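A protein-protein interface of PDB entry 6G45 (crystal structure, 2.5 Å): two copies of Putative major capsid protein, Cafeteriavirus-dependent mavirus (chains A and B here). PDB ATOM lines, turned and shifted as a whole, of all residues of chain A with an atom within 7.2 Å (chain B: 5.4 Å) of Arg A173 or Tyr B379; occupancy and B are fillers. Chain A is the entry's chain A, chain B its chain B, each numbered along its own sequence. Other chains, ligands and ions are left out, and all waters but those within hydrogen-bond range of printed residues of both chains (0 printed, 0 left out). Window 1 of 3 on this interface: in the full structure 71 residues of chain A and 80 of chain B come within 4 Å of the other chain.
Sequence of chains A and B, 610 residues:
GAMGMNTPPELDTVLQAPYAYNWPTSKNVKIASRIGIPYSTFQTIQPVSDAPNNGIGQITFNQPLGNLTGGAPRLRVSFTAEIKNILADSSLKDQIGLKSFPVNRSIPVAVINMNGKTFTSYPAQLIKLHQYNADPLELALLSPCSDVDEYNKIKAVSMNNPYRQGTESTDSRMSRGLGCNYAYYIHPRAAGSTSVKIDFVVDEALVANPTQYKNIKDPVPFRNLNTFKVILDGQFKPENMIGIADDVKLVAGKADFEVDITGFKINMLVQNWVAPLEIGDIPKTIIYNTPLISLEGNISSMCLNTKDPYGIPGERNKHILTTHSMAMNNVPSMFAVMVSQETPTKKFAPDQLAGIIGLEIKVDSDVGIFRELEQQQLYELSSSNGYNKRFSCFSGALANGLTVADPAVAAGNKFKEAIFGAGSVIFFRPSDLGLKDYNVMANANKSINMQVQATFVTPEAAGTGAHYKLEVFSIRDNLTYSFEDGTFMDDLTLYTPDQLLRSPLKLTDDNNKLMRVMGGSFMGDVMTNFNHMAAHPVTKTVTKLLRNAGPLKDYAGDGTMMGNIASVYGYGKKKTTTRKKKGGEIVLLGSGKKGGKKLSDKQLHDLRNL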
ATOM      1  N   TYR A  39     -42.550  19.213 -14.192  1.00  0.00           N
ATOM      2  CA  TYR A  39     -41.735  19.569 -13.024  1.00  0.00           C
ATOM      3  C   TYR A  39     -42.479  20.476 -12.024  1.00  0.00           C
ATOM      4  O   TYR A  39     -41.876  20.988 -11.082  1.00  0.00           O
ATOM      5  CB  TYR A  39     -40.415  20.208 -13.489  1.00  0.00           C
ATOM      6  CG  TYR A  39     -39.392  19.183 -13.934  1.00  0.00           C
ATOM      7  CD1 TYR A  39     -39.537  18.507 -15.148  1.00  0.00           C
ATOM      8  CD2 TYR A  39     -38.284  18.877 -13.141  1.00  0.00           C
ATOM      9  CE1 TYR A  39     -38.610  17.557 -15.557  1.00  0.00           C
ATOM     10  CE2 TYR A  39     -37.353  17.928 -13.542  1.00  0.00           C
ATOM     11  CZ  TYR A  39     -37.521  17.272 -14.749  1.00  0.00           C
ATOM     12  OH  TYR A  39     -36.600  16.336 -15.152  1.00  0.00           O
ATOM     13  N   PRO A 136     -22.257   3.894 -14.440  1.00  0.00           N
ATOM     14  CA  PRO A 136     -21.915   5.063 -13.612  1.00  0.00           C
ATOM     15  C   PRO A 136     -22.827   6.287 -13.783  1.00  0.00           C
ATOM     16  O   PRO A 136     -23.061   7.003 -12.811  1.00  0.00           O
ATOM     17  CB  PRO A 136     -20.489   5.399 -14.057  1.00  0.00           C
ATOM     18  CG  PRO A 136     -19.923   4.100 -14.497  1.00  0.00           C
ATOM     19  CD  PRO A 136     -21.062   3.344 -15.113  1.00  0.00           C
ATOM     20  N   LEU A 137     -23.327   6.517 -14.996  1.00  0.00           N
ATOM     21  CA  LEU A 137     -24.257   7.619 -15.260  1.00  0.00           C
ATOM     22  C   LEU A 137     -25.634   7.390 -14.626  1.00  0.00           C
ATOM     23  O   LEU A 137     -26.272   8.344 -14.181  1.00  0.00           O
ATOM     24  CB  LEU A 137     -24.395   7.866 -16.768  1.00  0.00           C
ATOM     25  CG  LEU A 137     -23.106   8.257 -17.508  1.00  0.00           C
ATOM     26  CD1 LEU A 137     -23.335   8.275 -19.014  1.00  0.00           C
ATOM     27  CD2 LEU A 137     -22.568   9.602 -17.032  1.00  0.00           C
ATOM     28  N   ALA A 140     -25.109   8.135 -10.896  1.00  0.00           N
ATOM     29  CA  ALA A 140     -25.034   9.576 -10.637  1.00  0.00           C
ATOM     30  C   ALA A 140     -26.412  10.241 -10.516  1.00  0.00           C
ATOM     31  O   ALA A 140     -26.540  11.289  -9.880  1.00  0.00           O
ATOM     32  CB  ALA A 140     -24.210  10.259 -11.717  1.00  0.00           C
ATOM     33  N   LEU A 141     -27.424   9.642 -11.140  1.00  0.00           N
ATOM     34  CA  LEU A 141     -28.815  10.063 -10.961  1.00  0.00           C
ATOM     35  C   LEU A 141     -29.430   9.592  -9.637  1.00  0.00           C
ATOM     36  O   LEU A 141     -30.351  10.237  -9.137  1.00  0.00           O
ATOM     37  CB  LEU A 141     -29.670   9.593 -12.141  1.00  0.00           C
ATOM     38  CG  LEU A 141     -29.269  10.131 -13.520  1.00  0.00           C
ATOM     39  CD1 LEU A 141     -30.141   9.487 -14.584  1.00  0.00           C
ATOM     40  CD2 LEU A 141     -29.357  11.651 -13.604  1.00  0.00           C
ATOM     41  N   SER A 143     -27.556   9.229  -6.696  1.00  0.00           N
ATOM     42  CA  SER A 143     -26.879   9.935  -5.607  1.00  0.00           C
ATOM     43  C   SER A 143     -25.845  10.947  -6.112  1.00  0.00           C
ATOM     44  O   SER A 143     -25.177  10.693  -7.118  1.00  0.00           O
ATOM     45  CB  SER A 143     -26.179   8.920  -4.698  1.00  0.00           C
ATOM     46  OG  SER A 143     -25.519   9.556  -3.618  1.00  0.00           O
ATOM     47  N   PRO A 144     -25.686  12.084  -5.393  1.00  0.00           N
ATOM     48  CA  PRO A 144     -24.595  13.012  -5.697  1.00  0.00           C
ATOM     49  C   PRO A 144     -23.207  12.500  -5.270  1.00  0.00           C
ATOM     50  O   PRO A 144     -22.203  13.121  -5.619  1.00  0.00           O
ATOM     51  CB  PRO A 144     -24.976  14.267  -4.901  1.00  0.00           C
ATOM     52  CG  PRO A 144     -25.751  13.751  -3.748  1.00  0.00           C
ATOM     53  CD  PRO A 144     -26.523  12.583  -4.284  1.00  0.00           C
ATOM     54  N   CYS A 145     -23.166  11.406  -4.505  1.00  0.00           N
ATOM     55  CA  CYS A 145     -21.926  10.735  -4.127  1.00  0.00           C
ATOM     56  C   CYS A 145     -21.900   9.316  -4.706  1.00  0.00           C
ATOM     57  O   CYS A 145     -21.821   8.329  -3.970  1.00  0.00           O
ATOM     58  CB  CYS A 145     -21.813  10.707  -2.603  1.00  0.00           C
ATOM     59  SG  CYS A 145     -21.907  12.340  -1.834  1.00  0.00           S
ATOM     60  N   SER A 146     -21.967   9.228  -6.032  1.00  0.00           N
ATOM     61  CA  SER A 146     -22.021   7.938  -6.734  1.00  0.00           C
ATOM     62  C   SER A 146     -20.658   7.274  -6.947  1.00  0.00           C
ATOM     63  O   SER A 146     -20.598   6.069  -7.193  1.00  0.00           O
ATOM     64  CB  SER A 146     -22.719   8.095  -8.086  1.00  0.00           C
ATOM     65  OG  SER A 146     -21.997   8.958  -8.945  1.00  0.00           O
ATOM     66  N   ASP A 147     -19.577   8.049  -6.867  1.00  0.00           N
ATOM     67  CA  ASP A 147     -18.239   7.518  -7.103  1.00  0.00           C
ATOM     68  C   ASP A 147     -17.834   6.525  -6.012  1.00  0.00           C
ATOM     69  O   ASP A 147     -17.913   6.830  -4.824  1.00  0.00           O
ATOM     70  CB  ASP A 147     -17.216   8.651  -7.180  1.00  0.00           C
ATOM     71  CG  ASP A 147     -15.850   8.173  -7.645  1.00  0.00           C
ATOM     72  OD1 ASP A 147     -15.760   7.567  -8.731  1.00  0.00           O
ATOM     73  OD2 ASP A 147     -14.861   8.413  -6.931  1.00  0.00           O
ATOM     74  N   SER A 169     -10.996  18.283  -9.323  1.00  0.00           N
ATOM     75  CA  SER A 169     -11.427  16.976  -9.836  1.00  0.00           C
ATOM     76  C   SER A 169     -11.342  16.913 -11.353  1.00  0.00           C
ATOM     77  O   SER A 169     -11.627  17.902 -12.035  1.00  0.00           O
ATOM     78  CB  SER A 169     -12.865  16.689  -9.414  1.00  0.00           C
ATOM     79  OG  SER A 169     -12.984  16.701  -8.005  1.00  0.00           O
ATOM     80  N   THR A 170     -10.955  15.751 -11.874  1.00  0.00           N
ATOM     81  CA  THR A 170     -10.983  15.497 -13.317  1.00  0.00           C
ATOM     82  C   THR A 170     -12.423  15.480 -13.851  1.00  0.00           C
ATOM     83  O   THR A 170     -12.673  15.893 -14.983  1.00  0.00           O
ATOM     84  CB  THR A 170     -10.294  14.164 -13.671  1.00  0.00           C
ATOM     85  OG1 THR A 170     -10.949  13.086 -12.997  1.00  0.00           O
ATOM     86  CG2 THR A 170      -8.828  14.191 -13.264  1.00  0.00           C
ATOM     87  N   ASP A 171     -13.347  14.997 -13.021  1.00  0.00           N
ATOM     88  CA  ASP A 171     -14.776  14.991 -13.315  1.00  0.00           C
ATOM     89  C   ASP A 171     -15.510  15.206 -11.988  1.00  0.00           C
ATOM     90  O   ASP A 171     -15.556  14.306 -11.150  1.00  0.00           O
ATOM     91  CB  ASP A 171     -15.173  13.650 -13.952  1.00  0.00           C
ATOM     92  CG  ASP A 171     -16.612  13.624 -14.464  1.00  0.00           C
ATOM     93  OD1 ASP A 171     -17.411  14.537 -14.145  1.00  0.00           O
ATOM     94  OD2 ASP A 171     -16.945  12.666 -15.194  1.00  0.00           O
ATOM     95  N   SER A 172     -16.072  16.402 -11.806  1.00  0.00           N
ATOM     96  CA  SER A 172     -16.723  16.773 -10.542  1.00  0.00           C
ATOM     97  C   SER A 172     -17.943  15.913 -10.206  1.00  0.00           C
ATOM     98  O   SER A 172     -18.239  15.710  -9.028  1.00  0.00           O
ATOM     99  CB  SER A 172     -17.106  18.259 -10.539  1.00  0.00           C
ATOM    100  OG  SER A 172     -18.159  18.535 -11.443  1.00  0.00           O
ATOM    101  N   ARG A 173     -18.644  15.415 -11.227  1.00  0.00           N
ATOM    102  CA  ARG A 173     -19.747  14.466 -11.027  1.00  0.00           C
ATOM    103  C   ARG A 173     -19.276  13.148 -10.403  1.00  0.00           C
ATOM    104  O   ARG A 173     -20.008  12.542  -9.626  1.00  0.00           O
ATOM    105  CB  ARG A 173     -20.479  14.185 -12.344  1.00  0.00           C
ATOM    106  CG  ARG A 173     -21.814  13.468 -12.179  1.00  0.00           C
ATOM    107  CD  ARG A 173     -22.419  13.051 -13.511  1.00  0.00           C
ATOM    108  NE  ARG A 173     -23.039  14.178 -14.213  1.00  0.00           N
ATOM    109  CZ  ARG A 173     -22.759  14.597 -15.453  1.00  0.00           C
ATOM    110  NH1 ARG A 173     -21.847  13.993 -16.223  1.00  0.00           N
ATOM    111  NH2 ARG A 173     -23.418  15.647 -15.943  1.00  0.00           N
ATOM    112  N   MET A 174     -18.056  12.725 -10.741  1.00  0.00           N
ATOM    113  CA  MET A 174     -17.444  11.507 -10.190  1.00  0.00           C
ATOM    114  C   MET A 174     -16.512  11.776  -8.998  1.00  0.00           C
ATOM    115  O   MET A 174     -15.543  11.046  -8.778  1.00  0.00           O
ATOM    116  CB  MET A 174     -16.690  10.769 -11.303  1.00  0.00           C
ATOM    117  CG  MET A 174     -17.559  10.388 -12.495  1.00  0.00           C
ATOM    118  SD  MET A 174     -18.985   9.372 -12.056  1.00  0.00           S
ATOM    119  CE  MET A 174     -18.145   7.899 -11.460  1.00  0.00           C
ATOM    120  N   SER A 175     -16.817  12.823  -8.232  1.00  0.00           N
ATOM    121  CA  SER A 175     -16.151  13.102  -6.971  1.00  0.00           C
ATOM    122  C   SER A 175     -17.202  13.213  -5.867  1.00  0.00           C
ATOM    123  O   SER A 175     -18.364  13.536  -6.126  1.00  0.00           O
ATOM    124  CB  SER A 175     -15.341  14.395  -7.071  1.00  0.00           C
ATOM    125  OG  SER A 175     -14.628  14.645  -5.871  1.00  0.00           O
ATOM    126  N   ARG A 176     -16.776  12.919  -4.643  1.00  0.00           N
ATOM    127  CA  ARG A 176     -17.597  13.071  -3.449  1.00  0.00           C
ATOM    128  C   ARG A 176     -17.107  14.239  -2.583  1.00  0.00           C
ATOM    129  O   ARG A 176     -17.514  14.371  -1.429  1.00  0.00           O
ATOM    130  CB  ARG A 176     -17.573  11.779  -2.628  1.00  0.00           C
ATOM    131  CG  ARG A 176     -17.830  10.505  -3.420  1.00  0.00           C
ATOM    132  CD  ARG A 176     -18.127   9.340  -2.485  1.00  0.00           C
ATOM    133  NE  ARG A 176     -16.999   9.034  -1.601  1.00  0.00           N
ATOM    134  CZ  ARG A 176     -16.010   8.167  -1.849  1.00  0.00           C
ATOM    135  NH1 ARG A 176     -15.955   7.463  -2.976  1.00  0.00           N
ATOM    136  NH2 ARG A 176     -15.052   8.000  -0.943  1.00  0.00           N
ATOM    137  N   CYS A 180     -18.878  19.937  -5.303  1.00  0.00           N
ATOM    138  CA  CYS A 180     -19.168  19.010  -6.390  1.00  0.00           C
ATOM    139  C   CYS A 180     -20.684  18.928  -6.587  1.00  0.00           C
ATOM    140  O   CYS A 180     -21.278  19.908  -7.031  1.00  0.00           O
ATOM    141  CB  CYS A 180     -18.507  17.655  -6.120  1.00  0.00           C
ATOM    142  SG  CYS A 180     -16.705  17.723  -6.191  1.00  0.00           S
ATOM    143  N   ASN A 181     -21.315  17.804  -6.237  1.00  0.00           N
ATOM    144  CA  ASN A 181     -22.724  17.560  -6.566  1.00  0.00           C
ATOM    145  C   ASN A 181     -23.715  17.941  -5.467  1.00  0.00           C
ATOM    146  O   ASN A 181     -24.907  18.062  -5.746  1.00  0.00           O
ATOM    147  CB  ASN A 181     -22.928  16.088  -6.926  1.00  0.00           C
ATOM    148  CG  ASN A 181     -22.098  15.657  -8.117  1.00  0.00           C
ATOM    149  OD1 ASN A 181     -21.928  16.414  -9.071  1.00  0.00           O
ATOM    150  ND2 ASN A 181     -21.573  14.438  -8.067  1.00  0.00           N
ATOM    151  N   GLU B 374     -36.137  23.799  -5.971  1.00  0.00           N
ATOM    152  CA  GLU B 374     -34.786  24.195  -5.549  1.00  0.00           C
ATOM    153  C   GLU B 374     -33.783  23.904  -6.672  1.00  0.00           C
ATOM    154  O   GLU B 374     -34.155  23.367  -7.718  1.00  0.00           O
ATOM    155  CB  GLU B 374     -34.390  23.453  -4.267  1.00  0.00           C
ATOM    156  CG  GLU B 374     -35.493  23.407  -3.210  1.00  0.00           C
ATOM    157  CD  GLU B 374     -34.979  23.188  -1.793  1.00  0.00           C
ATOM    158  OE1 GLU B 374     -33.887  22.602  -1.618  1.00  0.00           O
ATOM    159  OE2 GLU B 374     -35.680  23.597  -0.841  1.00  0.00           O
ATOM    160  N   GLN B 375     -32.518  24.261  -6.449  1.00  0.00           N
ATOM    161  CA  GLN B 375     -31.459  24.120  -7.458  1.00  0.00           C
ATOM    162  C   GLN B 375     -31.323  22.720  -8.058  1.00  0.00           C
ATOM    163  O   GLN B 375     -31.180  22.587  -9.270  1.00  0.00           O
ATOM    164  CB  GLN B 375     -30.104  24.554  -6.885  1.00  0.00           C
ATOM    165  CG  GLN B 375     -29.840  26.050  -6.962  1.00  0.00           C
ATOM    166  CD  GLN B 375     -28.368  26.379  -7.107  1.00  0.00           C
ATOM    167  OE1 GLN B 375     -27.524  25.779  -6.448  1.00  0.00           O
ATOM    168  NE2 GLN B 375     -28.052  27.331  -7.979  1.00  0.00           N
ATOM    169  N   GLN B 376     -31.357  21.693  -7.212  1.00  0.00           N
ATOM    170  CA  GLN B 376     -31.239  20.303  -7.669  1.00  0.00           C
ATOM    171  C   GLN B 376     -32.312  19.935  -8.693  1.00  0.00           C
ATOM    172  O   GLN B 376     -32.019  19.275  -9.689  1.00  0.00           O
ATOM    173  CB  GLN B 376     -31.307  19.334  -6.483  1.00  0.00           C
ATOM    174  CG  GLN B 376     -30.080  19.350  -5.579  1.00  0.00           C
ATOM    175  CD  GLN B 376     -28.827  18.772  -6.228  1.00  0.00           C
ATOM    176  OE1 GLN B 376     -28.882  18.143  -7.292  1.00  0.00           O
ATOM    177  NE2 GLN B 376     -27.685  18.984  -5.580  1.00  0.00           N
ATOM    178  N   GLN B 377     -33.542  20.374  -8.442  1.00  0.00           N
ATOM    179  CA  GLN B 377     -34.661  20.124  -9.349  1.00  0.00           C
ATOM    180  C   GLN B 377     -34.572  20.957 -10.629  1.00  0.00           C
ATOM    181  O   GLN B 377     -34.935  20.476 -11.700  1.00  0.00           O
ATOM    182  CB  GLN B 377     -35.998  20.372  -8.639  1.00  0.00           C
ATOM    183  CG  GLN B 377     -36.471  19.201  -7.787  1.00  0.00           C
ATOM    184  CD  GLN B 377     -35.614  18.986  -6.552  1.00  0.00           C
ATOM    185  OE1 GLN B 377     -35.562  19.842  -5.666  1.00  0.00           O
ATOM    186  NE2 GLN B 377     -34.931  17.842  -6.490  1.00  0.00           N
ATOM    187  N   LEU B 378     -34.099  22.198 -10.511  1.00  0.00           N
ATOM    188  CA  LEU B 378     -33.837  23.046 -11.677  1.00  0.00           C
ATOM    189  C   LEU B 378     -32.711  22.485 -12.558  1.00  0.00           C
ATOM    190  O   LEU B 378     -32.764  22.607 -13.785  1.00  0.00           O
ATOM    191  CB  LEU B 378     -33.501  24.476 -11.240  1.00  0.00           C
ATOM    192  CG  LEU B 378     -34.619  25.281 -10.569  1.00  0.00           C
ATOM    193  CD1 LEU B 378     -34.068  26.579  -9.998  1.00  0.00           C
ATOM    194  CD2 LEU B 378     -35.758  25.573 -11.531  1.00  0.00           C
ATOM    195  N   TYR B 379     -31.704  21.876 -11.930  1.00  0.00           N
ATOM    196  CA  TYR B 379     -30.625  21.197 -12.653  1.00  0.00           C
ATOM    197  C   TYR B 379     -31.134  19.976 -13.428  1.00  0.00           C
ATOM    198  O   TYR B 379     -30.755  19.778 -14.585  1.00  0.00           O
ATOM    199  CB  TYR B 379     -29.504  20.784 -11.691  1.00  0.00           C
ATOM    200  CG  TYR B 379     -28.415  19.965 -12.347  1.00  0.00           C
ATOM    201  CD1 TYR B 379     -27.573  20.535 -13.298  1.00  0.00           C
ATOM    202  CD2 TYR B 379     -28.232  18.617 -12.029  1.00  0.00           C
ATOM    203  CE1 TYR B 379     -26.578  19.791 -13.913  1.00  0.00           C
ATOM    204  CE2 TYR B 379     -27.237  17.864 -12.641  1.00  0.00           C
ATOM    205  CZ  TYR B 379     -26.414  18.459 -13.584  1.00  0.00           C
ATOM    206  OH  TYR B 379     -25.427  17.728 -14.195  1.00  0.00           O
ATOM    207  N   GLU B 380     -31.974  19.164 -12.781  1.00  0.00           N
ATOM    208  CA  GLU B 380     -32.616  18.010 -13.423  1.00  0.00           C
ATOM    209  C   GLU B 380     -33.497  18.415 -14.608  1.00  0.00           C
ATOM    210  O   GLU B 380     -33.476  17.757 -15.647  1.00  0.00           O
ATOM    211  CB  GLU B 380     -33.467  17.237 -12.412  1.00  0.00           C
ATOM    212  CG  GLU B 380     -32.680  16.406 -11.410  1.00  0.00           C
ATOM    213  CD  GLU B 380     -33.563  15.838 -10.305  1.00  0.00           C
ATOM    214  OE1 GLU B 380     -34.769  15.591 -10.558  1.00  0.00           O
ATOM    215  OE2 GLU B 380     -33.050  15.632  -9.180  1.00  0.00           O
ATOM    216  N   LEU B 381     -34.270  19.487 -14.432  1.00  0.00           N
ATOM    217  CA  LEU B 381     -35.108  20.052 -15.494  1.00  0.00           C
ATOM    218  C   LEU B 381     -34.278  20.382 -16.732  1.00  0.00           C
ATOM    219  O   LEU B 381     -34.593  19.932 -17.838  1.00  0.00           O
ATOM    220  CB  LEU B 381     -35.817  21.316 -14.986  1.00  0.00           C
ATOM    221  CG  LEU B 381     -36.612  22.176 -15.981  1.00  0.00           C
ATOM    222  CD1 LEU B 381     -37.705  21.367 -16.658  1.00  0.00           C
ATOM    223  CD2 LEU B 381     -37.204  23.388 -15.279  1.00  0.00           C
ATOM    224  N   SER B 382     -33.219  21.159 -16.526  1.00  0.00           N
ATOM    225  CA  SER B 382     -32.322  21.565 -17.605  1.00  0.00           C
ATOM    226  C   SER B 382     -31.586  20.379 -18.229  1.00  0.00           C
ATOM    227  O   SER B 382     -31.464  20.301 -19.451  1.00  0.00           O
ATOM    228  CB  SER B 382     -31.320  22.608 -17.102  1.00  0.00           C
ATOM    229  OG  SER B 382     -30.874  23.421 -18.171  1.00  0.00           O
ATOM    230  N   SER B 383     -31.114  19.461 -17.388  1.00  0.00           N
ATOM    231  CA  SER B 383     -30.439  18.242 -17.839  1.00  0.00           C
ATOM    232  C   SER B 383     -31.328  17.323 -18.683  1.00  0.00           C
ATOM    233  O   SER B 383     -30.860  16.743 -19.659  1.00  0.00           O
ATOM    234  CB  SER B 383     -29.883  17.477 -16.638  1.00  0.00           C
ATOM    235  OG  SER B 383     -28.948  18.276 -15.933  1.00  0.00           O
ATOM    236  N   SER B 384     -32.606  17.209 -18.323  1.00  0.00           N
ATOM    237  CA  SER B 384     -33.566  16.418 -19.107  1.00  0.00           C
ATOM    238  C   SER B 384     -33.874  17.021 -20.491  1.00  0.00           C
ATOM    239  O   SER B 384     -34.363  16.319 -21.375  1.00  0.00           O
ATOM    240  CB  SER B 384     -34.870  16.230 -18.323  1.00  0.00           C
ATOM    241  OG  SER B 384     -35.561  17.457 -18.174  1.00  0.00           O
ATOM    242  N   TYR B 387     -29.080  20.003 -21.213  1.00  0.00           N
ATOM    243  CA  TYR B 387     -27.989  20.705 -20.515  1.00  0.00           C
ATOM    244  C   TYR B 387     -26.798  19.775 -20.254  1.00  0.00           C
ATOM    245  O   TYR B 387     -26.962  18.707 -19.667  1.00  0.00           O
ATOM    246  CB  TYR B 387     -28.475  21.323 -19.206  1.00  0.00           C
ATOM    247  CG  TYR B 387     -27.426  22.157 -18.499  1.00  0.00           C
ATOM    248  CD1 TYR B 387     -27.116  23.442 -18.944  1.00  0.00           C
ATOM    249  CD2 TYR B 387     -26.736  21.661 -17.391  1.00  0.00           C
ATOM    250  CE1 TYR B 387     -26.150  24.209 -18.306  1.00  0.00           C
ATOM    251  CE2 TYR B 387     -25.768  22.421 -16.747  1.00  0.00           C
ATOM    252  CZ  TYR B 387     -25.480  23.696 -17.206  1.00  0.00           C
ATOM    253  OH  TYR B 387     -24.527  24.459 -16.573  1.00  0.00           O
ATOM    254  N   LYS B 389     -23.536  20.232 -18.795  1.00  0.00           N
ATOM    255  CA  LYS B 389     -22.524  20.465 -17.760  1.00  0.00           C
ATOM    256  C   LYS B 389     -22.985  19.916 -16.421  1.00  0.00           C
ATOM    257  O   LYS B 389     -24.141  19.529 -16.257  1.00  0.00           O
ATOM    258  CB  LYS B 389     -22.199  21.954 -17.649  1.00  0.00           C
ATOM    259  CG  LYS B 389     -21.909  22.602 -18.997  1.00  0.00           C
ATOM    260  CD  LYS B 389     -21.053  23.853 -18.891  1.00  0.00           C
ATOM    261  CE  LYS B 389     -19.594  23.551 -18.579  1.00  0.00           C
ATOM    262  NZ  LYS B 389     -18.982  22.558 -19.505  1.00  0.00           N
ATOM    263  N   ARG B 390     -22.057  19.880 -15.471  1.00  0.00           N
ATOM    264  CA  ARG B 390     -22.285  19.283 -14.158  1.00  0.00           C
ATOM    265  C   ARG B 390     -22.878  20.274 -13.158  1.00  0.00           C
ATOM    266  O   ARG B 390     -22.881  21.483 -13.397  1.00  0.00           O
ATOM    267  CB  ARG B 390     -20.970  18.704 -13.651  1.00  0.00           C
ATOM    268  CG  ARG B 390     -20.487  17.545 -14.518  1.00  0.00           C
ATOM    269  CD  ARG B 390     -19.000  17.587 -14.828  1.00  0.00           C
ATOM    270  NE  ARG B 390     -18.663  16.542 -15.800  1.00  0.00           N
ATOM    271  CZ  ARG B 390     -17.614  16.546 -16.632  1.00  0.00           C
ATOM    272  NH1 ARG B 390     -16.734  17.553 -16.652  1.00  0.00           N
ATOM    273  NH2 ARG B 390     -17.442  15.517 -17.464  1.00  0.00           N
ATOM    274  N   PHE B 391     -23.387  19.748 -12.045  1.00  0.00           N
ATOM    275  CA  PHE B 391     -24.029  20.574 -11.014  1.00  0.00           C
ATOM    276  C   PHE B 391     -23.077  21.591 -10.384  1.00  0.00           C
ATOM    277  O   PHE B 391     -23.485  22.714 -10.076  1.00  0.00           O
ATOM    278  CB  PHE B 391     -24.654  19.713  -9.913  1.00  0.00           C
ATOM    279  CG  PHE B 391     -25.394  20.515  -8.871  1.00  0.00           C
ATOM    280  CD1 PHE B 391     -26.679  20.982  -9.121  1.00  0.00           C
ATOM    281  CD2 PHE B 391     -24.796  20.826  -7.651  1.00  0.00           C
ATOM    282  CE1 PHE B 391     -27.362  21.733  -8.171  1.00  0.00           C
ATOM    283  CE2 PHE B 391     -25.474  21.575  -6.694  1.00  0.00           C
ATOM    284  CZ  PHE B 391     -26.759  22.029  -6.955  1.00  0.00           C
ATOM    285  N   PHE B 394     -23.284  24.407 -12.900  1.00  0.00           N
ATOM    286  CA  PHE B 394     -24.648  24.948 -12.958  1.00  0.00           C
ATOM    287  C   PHE B 394     -25.067  25.751 -11.722  1.00  0.00           C
ATOM    288  O   PHE B 394     -25.646  26.830 -11.849  1.00  0.00           O
ATOM    289  CB  PHE B 394     -25.645  23.801 -13.181  1.00  0.00           C
ATOM    290  CG  PHE B 394     -27.089  24.228 -13.154  1.00  0.00           C
ATOM    291  CD1 PHE B 394     -27.806  24.236 -11.960  1.00  0.00           C
ATOM    292  CD2 PHE B 394     -27.739  24.609 -14.322  1.00  0.00           C
ATOM    293  CE1 PHE B 394     -29.137  24.631 -11.933  1.00  0.00           C
ATOM    294  CE2 PHE B 394     -29.070  25.000 -14.300  1.00  0.00           C
ATOM    295  CZ  PHE B 394     -29.770  25.011 -13.104  1.00  0.00           C
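ND2 of Asn A181 is in hydrogen-bond range of O of Pro A144 (2.9 Å). The backbone NH of Arg A173 sits close to the side-chain carboxylate of Asp A171 (3.3 Å). OG of Ser A175 sits close to SG of Cys A180. O of Lys B389 lies within hydrogen-bond range of OH of Tyr B379. The backbone carbonyl oxygen (O) of Glu B380 lies within hydrogen-bond range of the side-chain hydroxyl (OG) of Ser B384, at 3.3 Å. The backbone carbonyl oxygen (O) of Leu B381 lies within hydrogen-bond range of the side-chain hydroxyl (OG) of Ser B384.
OH of Tyr A39 lies within hydrogen-bond range of O of Glu B380, at 3.5 Å. OH of Tyr A39 lies within hydrogen-bond range of OG of Ser B384 (3.4 Å). OD1 of Asp A171 is in salt-bridge range of NE of Arg B390, at 2.9 Å. NH2 of Arg A173 lies within hydrogen-bond range of OH of Tyr B379, at 3.4 Å. The backbone carbonyl oxygen (O) of Asn A181 is in hydrogen-bond range of the side-chain amide nitrogen (NE2) of Gln B376 (2.9 Å).
Of the printed residues of chain B, Arg A173 touches Tyr B379 (3.4 Å), Lys B389 (3.96 Å) and Arg B390 (3.8 Å). Of chain A, only Arg A173 comes within 4 Å of Tyr B379. Of the printed residues of chain A, Glu B380 touches Tyr A39 (3.5 Å). Of the printed residues of chain B, Asn A181 touches Gln B376 (2.9 Å) and Phe B391 (3.4 Å). Printed residues of chain B within 4 Å of Tyr A39: Gln B377, Glu B380, Leu B381 and Ser B384. Of the printed residues of chain A, Arg B390 touches Asp A171, Ser A172 and Arg A173. Ser A169 touches none of the printed residues of chain B. Cys A145 touches none of the printed residues of chain B. The nearest residue of chain A that does not touch Tyr B379 is Asn A181 (6.3 Å). The nearest printed residue of chain A that does not touch Phe B391 is Ser A172 (5.4 Å).
Of the 16 printed residues of chain B, 9 touch a printed residue of chain A. Hydrophobic or aromatic side chains of chain B that line the printed part of chain A: Tyr B379, Leu B381 and Phe B391. Hydrophobic or aromatic side chains of chain A that line the printed part of chain B: Tyr A39.
No position is printed for both chains.
Gln B377 touches Tyr A39. Tyr A39 touches Leu B381. Arg B390 touches Ser A172. O of Lys B389 touches NH2 of Arg A173 (3.96 Å). Arg B390 touches Arg A173 (CG to NH2, 3.8 Å). Cys A180 touches Phe B391. Asn A181 touches Phe B391 (O to CD2, 3.4 Å).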
